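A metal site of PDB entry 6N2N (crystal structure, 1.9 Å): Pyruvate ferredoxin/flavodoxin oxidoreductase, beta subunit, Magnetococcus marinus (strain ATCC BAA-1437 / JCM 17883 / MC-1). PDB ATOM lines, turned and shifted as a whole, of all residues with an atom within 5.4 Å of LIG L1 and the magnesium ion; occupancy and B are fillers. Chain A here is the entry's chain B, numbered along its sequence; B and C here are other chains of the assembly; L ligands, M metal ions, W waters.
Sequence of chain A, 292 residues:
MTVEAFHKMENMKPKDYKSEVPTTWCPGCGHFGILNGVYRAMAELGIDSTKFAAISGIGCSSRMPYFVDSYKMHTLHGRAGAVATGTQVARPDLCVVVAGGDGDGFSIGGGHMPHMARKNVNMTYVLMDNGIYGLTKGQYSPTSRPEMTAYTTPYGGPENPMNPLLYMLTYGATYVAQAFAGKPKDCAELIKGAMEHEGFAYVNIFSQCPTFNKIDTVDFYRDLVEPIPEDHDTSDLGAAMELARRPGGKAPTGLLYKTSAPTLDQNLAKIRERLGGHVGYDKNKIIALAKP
The side-chain amide nitrogen (ND2) of Asn 130 lies close to a sulfur (S4) of LG2 L2.
A sulfur (S1) of LIG L1 lies close to the backbone NH (N) of Gly 59 (3.6 Å).
The backbone NH (N) of Leu 135 is in hydrogen-bond range of an oxygen (O7) of LIG L1.
NE2 of His 31 lies within hydrogen-bond range of O5 of LIG L1.
N1 of LIG L1 is in hydrogen-bond range of OE1 of Glu 253 of chain B, 2.7 Å away.
The backbone NH (N) of Gly 134 lies within hydrogen-bond range of an oxygen (O7) of LIG L1 (3.2 Å).
An oxygen (O7) of LIG L1 sits close to the side-chain sulfur of Cys 60, 3.6 Å away.
O7 of LIG L1 is in hydrogen-bond range of N of Cys 60, at 2.8 Å.
O3 of LIG L1 sits close to N of Asp 102 (3.2 Å).
O5 of LIG L1 lies within hydrogen-bond range of N of Ser 61 (2.9 Å).
The backbone NH (N) of Asp 104 is in hydrogen-bond range of an oxygen (O2) of LIG L1, 2.7 Å away.
FE3 of LG2 L2 is bound by SG of Cys 60, at 2.3 Å.
The backbone NH (N) of Gly 103 sits at hydrogen-bond distance from an oxygen (O2) of LIG L1, at 3.4 Å.
NE2 of His 31 lies close to S4 of LG2 L2.
N of Ile 132 sits at hydrogen-bond distance from OG of Ser 141 (3.5 Å).
The side-chain sulfur (SG) of Cys 60 lies close to the backbone NH (N) of Leu 135, at 3.6 Å.
The backbone carbonyl oxygen (O) of Gly 100 sits close to the side-chain hydroxyl (OG) of Ser 61.
O of Gly 103 sits at hydrogen-bond distance from N of Ile 108 (3.4 Å).
SD of Met 128 sits at hydrogen-bond distance from OG of Ser 61, at 3.1 Å.
The side-chain carboxylate (OD1) of Asp 104 sits at hydrogen-bond distance from the backbone NH (N) of Ile 58.
OH of Tyr 224 of chain B sits at hydrogen-bond distance from NE2 of His 77, at 2.9 Å.
N of Ile 58 sits close to OG of Ser 62, 3.4 Å away.
O of Ile 58 sits close to S1 of LIG L1, at 3.5 Å.
NE2 of His 77 touches C9 of LIG L1, 3.3 Å away.
CA of Gly 101 touches O2 of LIG L1, at 3.6 Å.
CD1 of Ile 108 touches C2 of LIG L1, 3.8 Å away.
Tyr 133 touches LIG L1 (CA to O1, 3.4 Å).
Thr 136 touches LIG L1 (CG2 to N4, 3.4 Å).
Tyr 224 of chain B touches LIG L1.
Pro 225 of chain B touches LIG L1 (O to C5, 3.2 Å).
Ile 226 of chain B touches LIG L1 (CB to C5, 3.7 Å).
Leu 281 of chain B touches LIG L1 (CD1 to C2, 3.5 Å).
OE2 of Glu 284 of chain C touches C2 of LIG L1 (3.6 Å).
Hydrophobic or aromatic side chains within 4 Å of LIG L1: His 31, Ile 58, His 77, Ile 108, Tyr 133, Leu 135, Tyr 224 of chain B, Ile 226 of chain B and Leu 281 of chain B.
Within 4 Å of LIG L1: His 31, Ile 58, Gly 59, Cys 60, Ser 61, His 77, Gly 101, Asp 102, Gly 103, Asp 104, Ile 108, Asn 130, Ile 132, Tyr 133, Gly 134, Leu 135, Thr 136, Tyr 224 of chain B, Pro 225 of chain B, Ile 226 of chain B, Glu 253 of chain B, Leu 281 of chain B and Glu 284 of chain C.
Of the 33 residues printed, 3 come within 4 Å of the magnesium ion.
The magnesium ion is bound by OD1 of Asn 130, O3 of LIG L1, water W2, O6 of LIG L1, OD1 of Asp 102 and O of Ile 132.
Water W2 lies within hydrogen-bond range of O of Met 128 (2.8 Å), O5 of LIG L1 (2.9 Å) and ND2 of Asn 130 (3.1 Å).
Water W1 lies within hydrogen-bond range of OG of Ser 62, N of Gly 101, O2 of LIG L1 and O of Ile 58.
Water W3 lies within hydrogen-bond range of OE2 of Glu 284 of chain C (2.7 Å), N of His 77 (2.9 Å) and N2 of LIG L1 (3.0 Å).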
ATOM      1  N   HIS A  31       6.312 -18.239   4.748  1.00  0.00           N
ATOM      2  CA  HIS A  31       6.680 -18.567   6.122  1.00  0.00           C
ATOM      3  C   HIS A  31       5.797 -17.854   7.147  1.00  0.00           C
ATOM      4  O   HIS A  31       5.649 -18.350   8.264  1.00  0.00           O
ATOM      5  CB  HIS A  31       8.155 -18.237   6.376  1.00  0.00           C
ATOM      6  CG  HIS A  31       9.116 -19.029   5.546  1.00  0.00           C
ATOM      7  ND1 HIS A  31       8.760 -20.173   4.870  1.00  0.00           N
ATOM      8  CD2 HIS A  31      10.434 -18.822   5.265  1.00  0.00           C
ATOM      9  CE1 HIS A  31       9.817 -20.647   4.217  1.00  0.00           C
ATOM     10  NE2 HIS A  31      10.843 -19.847   4.448  1.00  0.00           N
ATOM     11  N   ILE A  58      19.907 -23.344   9.584  1.00  0.00           N
ATOM     12  CA  ILE A  58      20.122 -22.090   8.856  1.00  0.00           C
ATOM     13  C   ILE A  58      19.225 -22.074   7.621  1.00  0.00           C
ATOM     14  O   ILE A  58      19.043 -23.095   6.957  1.00  0.00           O
ATOM     15  CB  ILE A  58      21.595 -21.892   8.441  1.00  0.00           C
ATOM     16  CG1 ILE A  58      22.544 -22.114   9.627  1.00  0.00           C
ATOM     17  CG2 ILE A  58      21.806 -20.476   7.907  1.00  0.00           C
ATOM     18  CD1 ILE A  58      22.473 -21.033  10.668  1.00  0.00           C
ATOM     19  N   GLY A  59      18.664 -20.916   7.340  1.00  0.00           N
ATOM     20  CA  GLY A  59      17.729 -20.707   6.254  1.00  0.00           C
ATOM     21  C   GLY A  59      16.716 -19.656   6.670  1.00  0.00           C
ATOM     22  O   GLY A  59      16.602 -19.301   7.844  1.00  0.00           O
ATOM     23  N   CYS A  60      15.985 -19.134   5.686  1.00  0.00           N
ATOM     24  CA  CYS A  60      14.881 -18.224   6.009  1.00  0.00           C
ATOM     25  C   CYS A  60      13.882 -18.910   6.926  1.00  0.00           C
ATOM     26  O   CYS A  60      13.459 -18.352   7.944  1.00  0.00           O
ATOM     27  CB  CYS A  60      14.178 -17.752   4.731  1.00  0.00           C
ATOM     28  SG  CYS A  60      15.142 -16.611   3.704  1.00  0.00           S
ATOM     29  N   SER A  61      13.495 -20.146   6.584  1.00  0.00           N
ATOM     30  CA  SER A  61      12.614 -20.923   7.435  1.00  0.00           C
ATOM     31  C   SER A  61      13.139 -20.992   8.865  1.00  0.00           C
ATOM     32  O   SER A  61      12.398 -20.777   9.826  1.00  0.00           O
ATOM     33  CB  SER A  61      12.460 -22.334   6.867  1.00  0.00           C
ATOM     34  OG  SER A  61      11.721 -23.152   7.746  1.00  0.00           O
ATOM     35  N   SER A  62      14.452 -21.235   9.013  1.00  0.00           N
ATOM     36  CA  SER A  62      15.090 -21.481  10.293  1.00  0.00           C
ATOM     37  C   SER A  62      15.101 -20.268  11.214  1.00  0.00           C
ATOM     38  O   SER A  62      15.481 -20.401  12.380  1.00  0.00           O
ATOM     39  CB  SER A  62      16.530 -21.951  10.050  1.00  0.00           C
ATOM     40  OG  SER A  62      16.556 -23.122   9.251  1.00  0.00           O
ATOM     41  N   HIS A  77      23.657 -25.411  10.072  1.00  0.00           N
ATOM     42  CA  HIS A  77      22.882 -25.790   8.898  1.00  0.00           C
ATOM     43  C   HIS A  77      22.785 -27.314   8.789  1.00  0.00           C
ATOM     44  O   HIS A  77      23.802 -28.006   8.683  1.00  0.00           O
ATOM     45  CB  HIS A  77      23.547 -25.194   7.662  1.00  0.00           C
ATOM     46  CG  HIS A  77      22.773 -25.347   6.382  1.00  0.00           C
ATOM     47  ND1 HIS A  77      21.392 -25.273   6.325  1.00  0.00           N
ATOM     48  CD2 HIS A  77      23.191 -25.546   5.113  1.00  0.00           C
ATOM     49  CE1 HIS A  77      21.003 -25.443   5.073  1.00  0.00           C
ATOM     50  NE2 HIS A  77      22.077 -25.615   4.315  1.00  0.00           N
ATOM     51  N   GLY A 100      12.472 -25.745   9.844  1.00  0.00           N
ATOM     52  CA  GLY A 100      13.518 -25.550   8.861  1.00  0.00           C
ATOM     53  C   GLY A 100      12.981 -25.795   7.461  1.00  0.00           C
ATOM     54  O   GLY A 100      11.878 -26.312   7.284  1.00  0.00           O
ATOM     55  N   GLY A 101      13.815 -25.451   6.477  1.00  0.00           N
ATOM     56  CA  GLY A 101      13.405 -25.484   5.097  1.00  0.00           C
ATOM     57  C   GLY A 101      13.778 -26.776   4.386  1.00  0.00           C
ATOM     58  O   GLY A 101      14.298 -27.722   4.967  1.00  0.00           O
ATOM     59  N   ASP A 102      13.492 -26.796   3.080  1.00  0.00           N
ATOM     60  CA  ASP A 102      13.715 -28.014   2.313  1.00  0.00           C
ATOM     61  C   ASP A 102      15.199 -28.318   2.123  1.00  0.00           C
ATOM     62  O   ASP A 102      15.596 -29.491   2.113  1.00  0.00           O
ATOM     63  CB  ASP A 102      12.988 -27.922   0.961  1.00  0.00           C
ATOM     64  CG  ASP A 102      13.073 -26.528   0.323  1.00  0.00           C
ATOM     65  OD1 ASP A 102      12.948 -25.502   1.023  1.00  0.00           O
ATOM     66  OD2 ASP A 102      13.257 -26.479  -0.909  1.00  0.00           O
ATOM     67  N   GLY A 103      16.043 -27.286   1.990  1.00  0.00           N
ATOM     68  CA  GLY A 103      17.462 -27.538   1.855  1.00  0.00           C
ATOM     69  C   GLY A 103      18.125 -27.922   3.169  1.00  0.00           C
ATOM     70  O   GLY A 103      18.899 -28.893   3.242  1.00  0.00           O
ATOM     71  N   ASP A 104      17.824 -27.155   4.214  1.00  0.00           N
ATOM     72  CA  ASP A 104      18.317 -27.459   5.547  1.00  0.00           C
ATOM     73  C   ASP A 104      17.948 -28.880   5.978  1.00  0.00           C
ATOM     74  O   ASP A 104      18.759 -29.576   6.602  1.00  0.00           O
ATOM     75  CB  ASP A 104      17.758 -26.425   6.526  1.00  0.00           C
ATOM     76  CG  ASP A 104      18.247 -26.626   7.945  1.00  0.00           C
ATOM     77  OD1 ASP A 104      19.381 -26.218   8.255  1.00  0.00           O
ATOM     78  OD2 ASP A 104      17.474 -27.162   8.769  1.00  0.00           O
ATOM     79  N   GLY A 105      16.735 -29.316   5.649  1.00  0.00           N
ATOM     80  CA  GLY A 105      16.238 -30.603   6.097  1.00  0.00           C
ATOM     81  C   GLY A 105      16.674 -31.793   5.256  1.00  0.00           C
ATOM     82  O   GLY A 105      17.035 -32.841   5.793  1.00  0.00           O
ATOM     83  N   ILE A 108      21.706 -30.876   3.232  1.00  0.00           N
ATOM     84  CA  ILE A 108      22.740 -31.104   4.233  1.00  0.00           C
ATOM     85  C   ILE A 108      22.187 -31.855   5.449  1.00  0.00           C
ATOM     86  O   ILE A 108      22.916 -32.597   6.105  1.00  0.00           O
ATOM     87  CB  ILE A 108      23.387 -29.773   4.649  1.00  0.00           C
ATOM     88  CG1 ILE A 108      24.576 -30.015   5.575  1.00  0.00           C
ATOM     89  CG2 ILE A 108      22.345 -28.848   5.291  1.00  0.00           C
ATOM     90  CD1 ILE A 108      25.471 -28.814   5.753  1.00  0.00           C
ATOM     91  N   MET A 128       9.284 -26.325   6.052  1.00  0.00           N
ATOM     92  CA  MET A 128       8.685 -25.254   5.268  1.00  0.00           C
ATOM     93  C   MET A 128       9.248 -25.329   3.850  1.00  0.00           C
ATOM     94  O   MET A 128      10.333 -24.827   3.576  1.00  0.00           O
ATOM     95  CB  MET A 128       8.957 -23.915   5.936  1.00  0.00           C
ATOM     96  CG  MET A 128       8.697 -23.960   7.430  1.00  0.00           C
ATOM     97  SD  MET A 128       8.756 -22.347   8.217  1.00  0.00           S
ATOM     98  CE  MET A 128       9.182 -22.839   9.864  1.00  0.00           C
ATOM     99  N   ASN A 130       9.650 -24.496   0.223  1.00  0.00           N
ATOM    100  CA  ASN A 130       9.466 -23.470  -0.792  1.00  0.00           C
ATOM    101  C   ASN A 130      10.142 -23.822  -2.120  1.00  0.00           C
ATOM    102  O   ASN A 130      10.157 -22.996  -3.029  1.00  0.00           O
ATOM    103  CB  ASN A 130       9.944 -22.086  -0.306  1.00  0.00           C
ATOM    104  CG  ASN A 130      11.375 -22.081   0.173  1.00  0.00           C
ATOM    105  OD1 ASN A 130      12.130 -23.023  -0.068  1.00  0.00           O
ATOM    106  ND2 ASN A 130      11.754 -20.993   0.853  1.00  0.00           N
ATOM    107  N   GLY A 131      10.679 -25.036  -2.238  1.00  0.00           N
ATOM    108  CA  GLY A 131      11.252 -25.484  -3.492  1.00  0.00           C
ATOM    109  C   GLY A 131      12.501 -24.745  -3.921  1.00  0.00           C
ATOM    110  O   GLY A 131      12.794 -24.698  -5.118  1.00  0.00           O
ATOM    111  N   ILE A 132      13.241 -24.170  -2.982  1.00  0.00           N
ATOM    112  CA  ILE A 132      14.404 -23.350  -3.308  1.00  0.00           C
ATOM    113  C   ILE A 132      15.223 -23.092  -2.047  1.00  0.00           C
ATOM    114  O   ILE A 132      14.742 -23.321  -0.930  1.00  0.00           O
ATOM    115  CB  ILE A 132      13.959 -22.039  -3.985  1.00  0.00           C
ATOM    116  CG1 ILE A 132      15.075 -21.464  -4.867  1.00  0.00           C
ATOM    117  CG2 ILE A 132      13.474 -21.027  -2.948  1.00  0.00           C
ATOM    118  CD1 ILE A 132      14.588 -20.481  -5.911  1.00  0.00           C
ATOM    119  N   TYR A 133      16.468 -22.629  -2.210  1.00  0.00           N
ATOM    120  CA  TYR A 133      17.247 -22.084  -1.091  1.00  0.00           C
ATOM    121  C   TYR A 133      17.016 -20.577  -1.064  1.00  0.00           C
ATOM    122  O   TYR A 133      17.595 -19.839  -1.859  1.00  0.00           O
ATOM    123  CB  TYR A 133      18.728 -22.382  -1.245  1.00  0.00           C
ATOM    124  CG  TYR A 133      19.135 -23.841  -1.287  1.00  0.00           C
ATOM    125  CD1 TYR A 133      18.240 -24.849  -0.956  1.00  0.00           C
ATOM    126  CD2 TYR A 133      20.428 -24.207  -1.646  1.00  0.00           C
ATOM    127  CE1 TYR A 133      18.633 -26.191  -0.998  1.00  0.00           C
ATOM    128  CE2 TYR A 133      20.828 -25.534  -1.689  1.00  0.00           C
ATOM    129  CZ  TYR A 133      19.916 -26.516  -1.370  1.00  0.00           C
ATOM    130  OH  TYR A 133      20.319 -27.830  -1.407  1.00  0.00           O
ATOM    131  N   GLY A 134      16.194 -20.130  -0.120  1.00  0.00           N
ATOM    132  CA  GLY A 134      15.892 -18.699  -0.041  1.00  0.00           C
ATOM    133  C   GLY A 134      17.037 -17.890   0.526  1.00  0.00           C
ATOM    134  O   GLY A 134      17.473 -16.904  -0.084  1.00  0.00           O
ATOM    135  N   LEU A 135      17.554 -18.291   1.690  1.00  0.00           N
ATOM    136  CA  LEU A 135      18.454 -17.423   2.445  1.00  0.00           C
ATOM    137  C   LEU A 135      19.757 -17.170   1.689  1.00  0.00           C
ATOM    138  O   LEU A 135      20.316 -16.069   1.773  1.00  0.00           O
ATOM    139  CB  LEU A 135      18.743 -17.997   3.826  1.00  0.00           C
ATOM    140  CG  LEU A 135      19.579 -17.098   4.738  1.00  0.00           C
ATOM    141  CD1 LEU A 135      18.883 -15.751   4.974  1.00  0.00           C
ATOM    142  CD2 LEU A 135      19.884 -17.783   6.061  1.00  0.00           C
ATOM    143  N   THR A 136      20.252 -18.157   0.946  1.00  0.00           N
ATOM    144  CA  THR A 136      21.461 -17.995   0.139  1.00  0.00           C
ATOM    145  C   THR A 136      21.188 -17.369  -1.225  1.00  0.00           C
ATOM    146  O   THR A 136      22.092 -17.351  -2.066  1.00  0.00           O
ATOM    147  CB  THR A 136      22.180 -19.336  -0.022  1.00  0.00           C
ATOM    148  OG1 THR A 136      21.228 -20.348  -0.365  1.00  0.00           O
ATOM    149  CG2 THR A 136      22.843 -19.707   1.284  1.00  0.00           C
ATOM    150  N   SER A 141      16.780 -26.700  -4.847  1.00  0.00           N
ATOM    151  CA  SER A 141      16.719 -27.584  -3.697  1.00  0.00           C
ATOM    152  C   SER A 141      16.286 -28.971  -4.135  1.00  0.00           C
ATOM    153  O   SER A 141      15.916 -29.185  -5.296  1.00  0.00           O
ATOM    154  CB  SER A 141      15.728 -27.018  -2.669  1.00  0.00           C
ATOM    155  OG  SER A 141      14.403 -27.438  -2.945  1.00  0.00           O
ATOM    156  N   TYR B 224      28.492 -26.576  -2.746  1.00  0.00           N
ATOM    157  CA  TYR B 224      27.254 -26.373  -2.020  1.00  0.00           C
ATOM    158  C   TYR B 224      27.191 -24.884  -1.689  1.00  0.00           C
ATOM    159  O   TYR B 224      28.210 -24.295  -1.301  1.00  0.00           O
ATOM    160  CB  TYR B 224      27.235 -27.235  -0.742  1.00  0.00           C
ATOM    161  CG  TYR B 224      25.900 -27.275  -0.019  1.00  0.00           C
ATOM    162  CD1 TYR B 224      24.786 -27.850  -0.612  1.00  0.00           C
ATOM    163  CD2 TYR B 224      25.781 -26.750   1.253  1.00  0.00           C
ATOM    164  CE1 TYR B 224      23.575 -27.887   0.048  1.00  0.00           C
ATOM    165  CE2 TYR B 224      24.577 -26.796   1.926  1.00  0.00           C
ATOM    166  CZ  TYR B 224      23.480 -27.361   1.323  1.00  0.00           C
ATOM    167  OH  TYR B 224      22.289 -27.401   1.993  1.00  0.00           O
ATOM    168  N   PRO B 225      26.055 -24.237  -1.897  1.00  0.00           N
ATOM    169  CA  PRO B 225      25.997 -22.778  -1.718  1.00  0.00           C
ATOM    170  C   PRO B 225      26.306 -22.396  -0.273  1.00  0.00           C
ATOM    171  O   PRO B 225      25.831 -23.024   0.671  1.00  0.00           O
ATOM    172  CB  PRO B 225      24.550 -22.426  -2.093  1.00  0.00           C
ATOM    173  CG  PRO B 225      24.090 -23.553  -2.942  1.00  0.00           C
ATOM    174  CD  PRO B 225      24.786 -24.787  -2.421  1.00  0.00           C
ATOM    175  N   ILE B 226      27.105 -21.345  -0.122  1.00  0.00           N
ATOM    176  CA  ILE B 226      27.377 -20.743   1.182  1.00  0.00           C
ATOM    177  C   ILE B 226      27.901 -19.339   0.965  1.00  0.00           C
ATOM    178  O   ILE B 226      28.726 -19.087   0.085  1.00  0.00           O
ATOM    179  CB  ILE B 226      28.364 -21.603   2.011  1.00  0.00           C
ATOM    180  CG1 ILE B 226      28.504 -21.025   3.437  1.00  0.00           C
ATOM    181  CG2 ILE B 226      29.727 -21.700   1.335  1.00  0.00           C
ATOM    182  CD1 ILE B 226      29.378 -21.884   4.347  1.00  0.00           C
ATOM    183  N   THR B 227      27.410 -18.414   1.794  1.00  0.00           N
ATOM    184  CA  THR B 227      27.899 -17.046   1.773  1.00  0.00           C
ATOM    185  C   THR B 227      29.285 -16.979   2.420  1.00  0.00           C
ATOM    186  O   THR B 227      29.519 -17.628   3.438  1.00  0.00           O
ATOM    187  CB  THR B 227      26.910 -16.138   2.534  1.00  0.00           C
ATOM    188  OG1 THR B 227      25.634 -16.230   1.915  1.00  0.00           O
ATOM    189  CG2 THR B 227      27.346 -14.676   2.544  1.00  0.00           C
ATOM    190  N   GLU B 253      28.891 -30.011   1.733  1.00  0.00           N
ATOM    191  CA  GLU B 253      30.300 -29.813   1.440  1.00  0.00           C
ATOM    192  C   GLU B 253      31.080 -31.116   1.460  1.00  0.00           C
ATOM    193  O   GLU B 253      32.050 -31.276   0.710  1.00  0.00           O
ATOM    194  CB  GLU B 253      30.932 -28.836   2.437  1.00  0.00           C
ATOM    195  CG  GLU B 253      30.536 -27.394   2.224  1.00  0.00           C
ATOM    196  CD  GLU B 253      29.256 -27.020   2.956  1.00  0.00           C
ATOM    197  OE1 GLU B 253      28.896 -25.834   2.907  1.00  0.00           O
ATOM    198  OE2 GLU B 253      28.641 -27.909   3.587  1.00  0.00           O
ATOM    199  N   PRO B 277      32.846 -22.564   7.533  1.00  0.00           N
ATOM    200  CA  PRO B 277      32.081 -23.761   7.949  1.00  0.00           C
ATOM    201  C   PRO B 277      32.242 -24.927   6.999  1.00  0.00           C
ATOM    202  O   PRO B 277      32.387 -26.081   7.446  1.00  0.00           O
ATOM    203  CB  PRO B 277      30.635 -23.243   7.990  1.00  0.00           C
ATOM    204  CG  PRO B 277      30.767 -21.757   8.237  1.00  0.00           C
ATOM    205  CD  PRO B 277      32.006 -21.348   7.505  1.00  0.00           C
ATOM    206  N   GLY B 278      32.245 -24.661   5.699  1.00  0.00           N
ATOM    207  CA  GLY B 278      32.403 -25.736   4.733  1.00  0.00           C
ATOM    208  C   GLY B 278      33.786 -26.339   4.757  1.00  0.00           C
ATOM    209  O   GLY B 278      33.936 -27.564   4.649  1.00  0.00           O
ATOM    210  N   LEU B 281      33.999 -28.833   7.523  1.00  0.00           N
ATOM    211  CA  LEU B 281      33.392 -30.117   7.184  1.00  0.00           C
ATOM    212  C   LEU B 281      34.266 -30.933   6.236  1.00  0.00           C
ATOM    213  O   LEU B 281      34.207 -32.167   6.272  1.00  0.00           O
ATOM    214  CB  LEU B 281      32.010 -29.903   6.574  1.00  0.00           C
ATOM    215  CG  LEU B 281      30.941 -29.384   7.541  1.00  0.00           C
ATOM    216  CD1 LEU B 281      29.723 -28.922   6.769  1.00  0.00           C
ATOM    217  CD2 LEU B 281      30.573 -30.493   8.529  1.00  0.00           C
ATOM    218  N   ARG B 303      35.070 -15.682   5.817  1.00  0.00           N
ATOM    219  CA  ARG B 303      34.066 -14.786   6.372  1.00  0.00           C
ATOM    220  C   ARG B 303      34.281 -14.674   7.878  1.00  0.00           C
ATOM    221  O   ARG B 303      35.204 -15.284   8.440  1.00  0.00           O
ATOM    222  CB  ARG B 303      32.646 -15.287   6.059  1.00  0.00           C
ATOM    223  CG  ARG B 303      32.230 -16.518   6.864  1.00  0.00           C
ATOM    224  CD  ARG B 303      30.941 -17.146   6.346  1.00  0.00           C
ATOM    225  NE  ARG B 303      30.164 -17.774   7.410  1.00  0.00           N
ATOM    226  CZ  ARG B 303      28.961 -18.320   7.226  1.00  0.00           C
ATOM    227  NH1 ARG B 303      28.426 -18.343   6.009  1.00  0.00           N
ATOM    228  NH2 ARG B 303      28.290 -18.843   8.245  1.00  0.00           N
ATOM    229  N   GLU C 284      33.254 -28.555  12.776  1.00  0.00           N
ATOM    230  CA  GLU C 284      32.257 -27.493  12.661  1.00  0.00           C
ATOM    231  C   GLU C 284      31.433 -27.372  13.938  1.00  0.00           C
ATOM    232  O   GLU C 284      31.241 -26.275  14.470  1.00  0.00           O
ATOM    233  CB  GLU C 284      31.342 -27.716  11.456  1.00  0.00           C
ATOM    234  CG  GLU C 284      30.707 -26.385  10.971  1.00  0.00           C
ATOM    235  CD  GLU C 284      29.336 -26.533  10.301  1.00  0.00           C
ATOM    236  OE1 GLU C 284      28.826 -27.662  10.185  1.00  0.00           O
ATOM    237  OE2 GLU C 284      28.778 -25.487   9.906  1.00  0.00           O
HETATM  238  N1  LIG L   1      26.867 -24.958   4.379  1.00  0.00           N
HETATM  239  C1  LIG L   1      27.001 -24.870   5.686  1.00  0.00           C
HETATM  240  C2  LIG L   1      27.847 -25.931   6.418  1.00  0.00           C
HETATM  241  N2  LIG L   1      26.413 -23.915   6.376  1.00  0.00           N
HETATM  242  C3  LIG L   1      25.666 -22.972   5.763  1.00  0.00           C
HETATM  243  N3  LIG L   1      25.058 -21.945   6.543  1.00  0.00           N
HETATM  244  C4  LIG L   1      25.488 -23.029   4.371  1.00  0.00           C
HETATM  245  C5  LIG L   1      26.142 -24.074   3.683  1.00  0.00           C
HETATM  246  C6  LIG L   1      24.644 -21.971   3.566  1.00  0.00           C
HETATM  247  N4  LIG L   1      23.224 -22.034   3.664  1.00  0.00           N
HETATM  248  C7  LIG L   1      22.434 -21.317   4.561  1.00  0.00           C
HETATM  249  S1  LIG L   1      20.814 -21.488   4.456  1.00  0.00           S
HETATM  250  C8  LIG L   1      21.063 -22.513   3.210  1.00  0.00           C
HETATM  251  C9  LIG L   1      22.390 -22.735   2.841  1.00  0.00           C
HETATM  252  C10 LIG L   1      22.818 -23.654   1.700  1.00  0.00           C
HETATM  253  C11 LIG L   1      19.876 -23.162   2.511  1.00  0.00           C
HETATM  254  C12 LIG L   1      18.533 -22.416   2.758  1.00  0.00           C
HETATM  255  O1  LIG L   1      17.505 -23.165   2.085  1.00  0.00           O
HETATM  256  P1  LIG L   1      16.302 -23.735   2.920  1.00  0.00           P
HETATM  257  O2  LIG L   1      16.761 -24.690   3.985  1.00  0.00           O
HETATM  258  O3  LIG L   1      15.374 -24.440   1.959  1.00  0.00           O
HETATM  259  O4  LIG L   1      15.552 -22.580   3.706  1.00  0.00           O
HETATM  260  P2  LIG L   1      14.854 -21.299   3.033  1.00  0.00           P
HETATM  261  O5  LIG L   1      13.636 -21.027   3.869  1.00  0.00           O
HETATM  262  O6  LIG L   1      14.518 -21.640   1.600  1.00  0.00           O
HETATM  263  O7  LIG L   1      15.816 -20.142   3.075  1.00  0.00           O
HETATM  264 FE1  LG2 L   2      12.091 -16.298  -0.019  1.00  0.00          FE
HETATM  265 FE2  LG2 L   2      10.691 -15.802   2.290  1.00  0.00          FE
HETATM  266 FE3  LG2 L   2      13.426 -15.925   2.338  1.00  0.00          FE
HETATM  267 FE4  LG2 L   2      12.161 -13.808   1.160  1.00  0.00          FE
HETATM  268  S1  LG2 L   2      12.101 -14.368   3.367  1.00  0.00           S
HETATM  269  S2  LG2 L   2      13.931 -15.003   0.328  1.00  0.00           S
HETATM  270  S3  LG2 L   2      10.342 -14.826   0.255  1.00  0.00           S
HETATM  271  S4  LG2 L   2      11.986 -17.630   1.829  1.00  0.00           S
HETATM  272 MG    MG M   1      13.784 -23.533   1.003  1.00  0.00          MG
HETATM  273  O   HOH W   1      15.953 -23.629   6.613  1.00  0.00           O
HETATM  274  O   HOH W   2      12.486 -23.397   2.625  1.00  0.00           O
HETATM  275  O   HOH W   3      26.311 -24.428   9.328  1.00  0.00           O
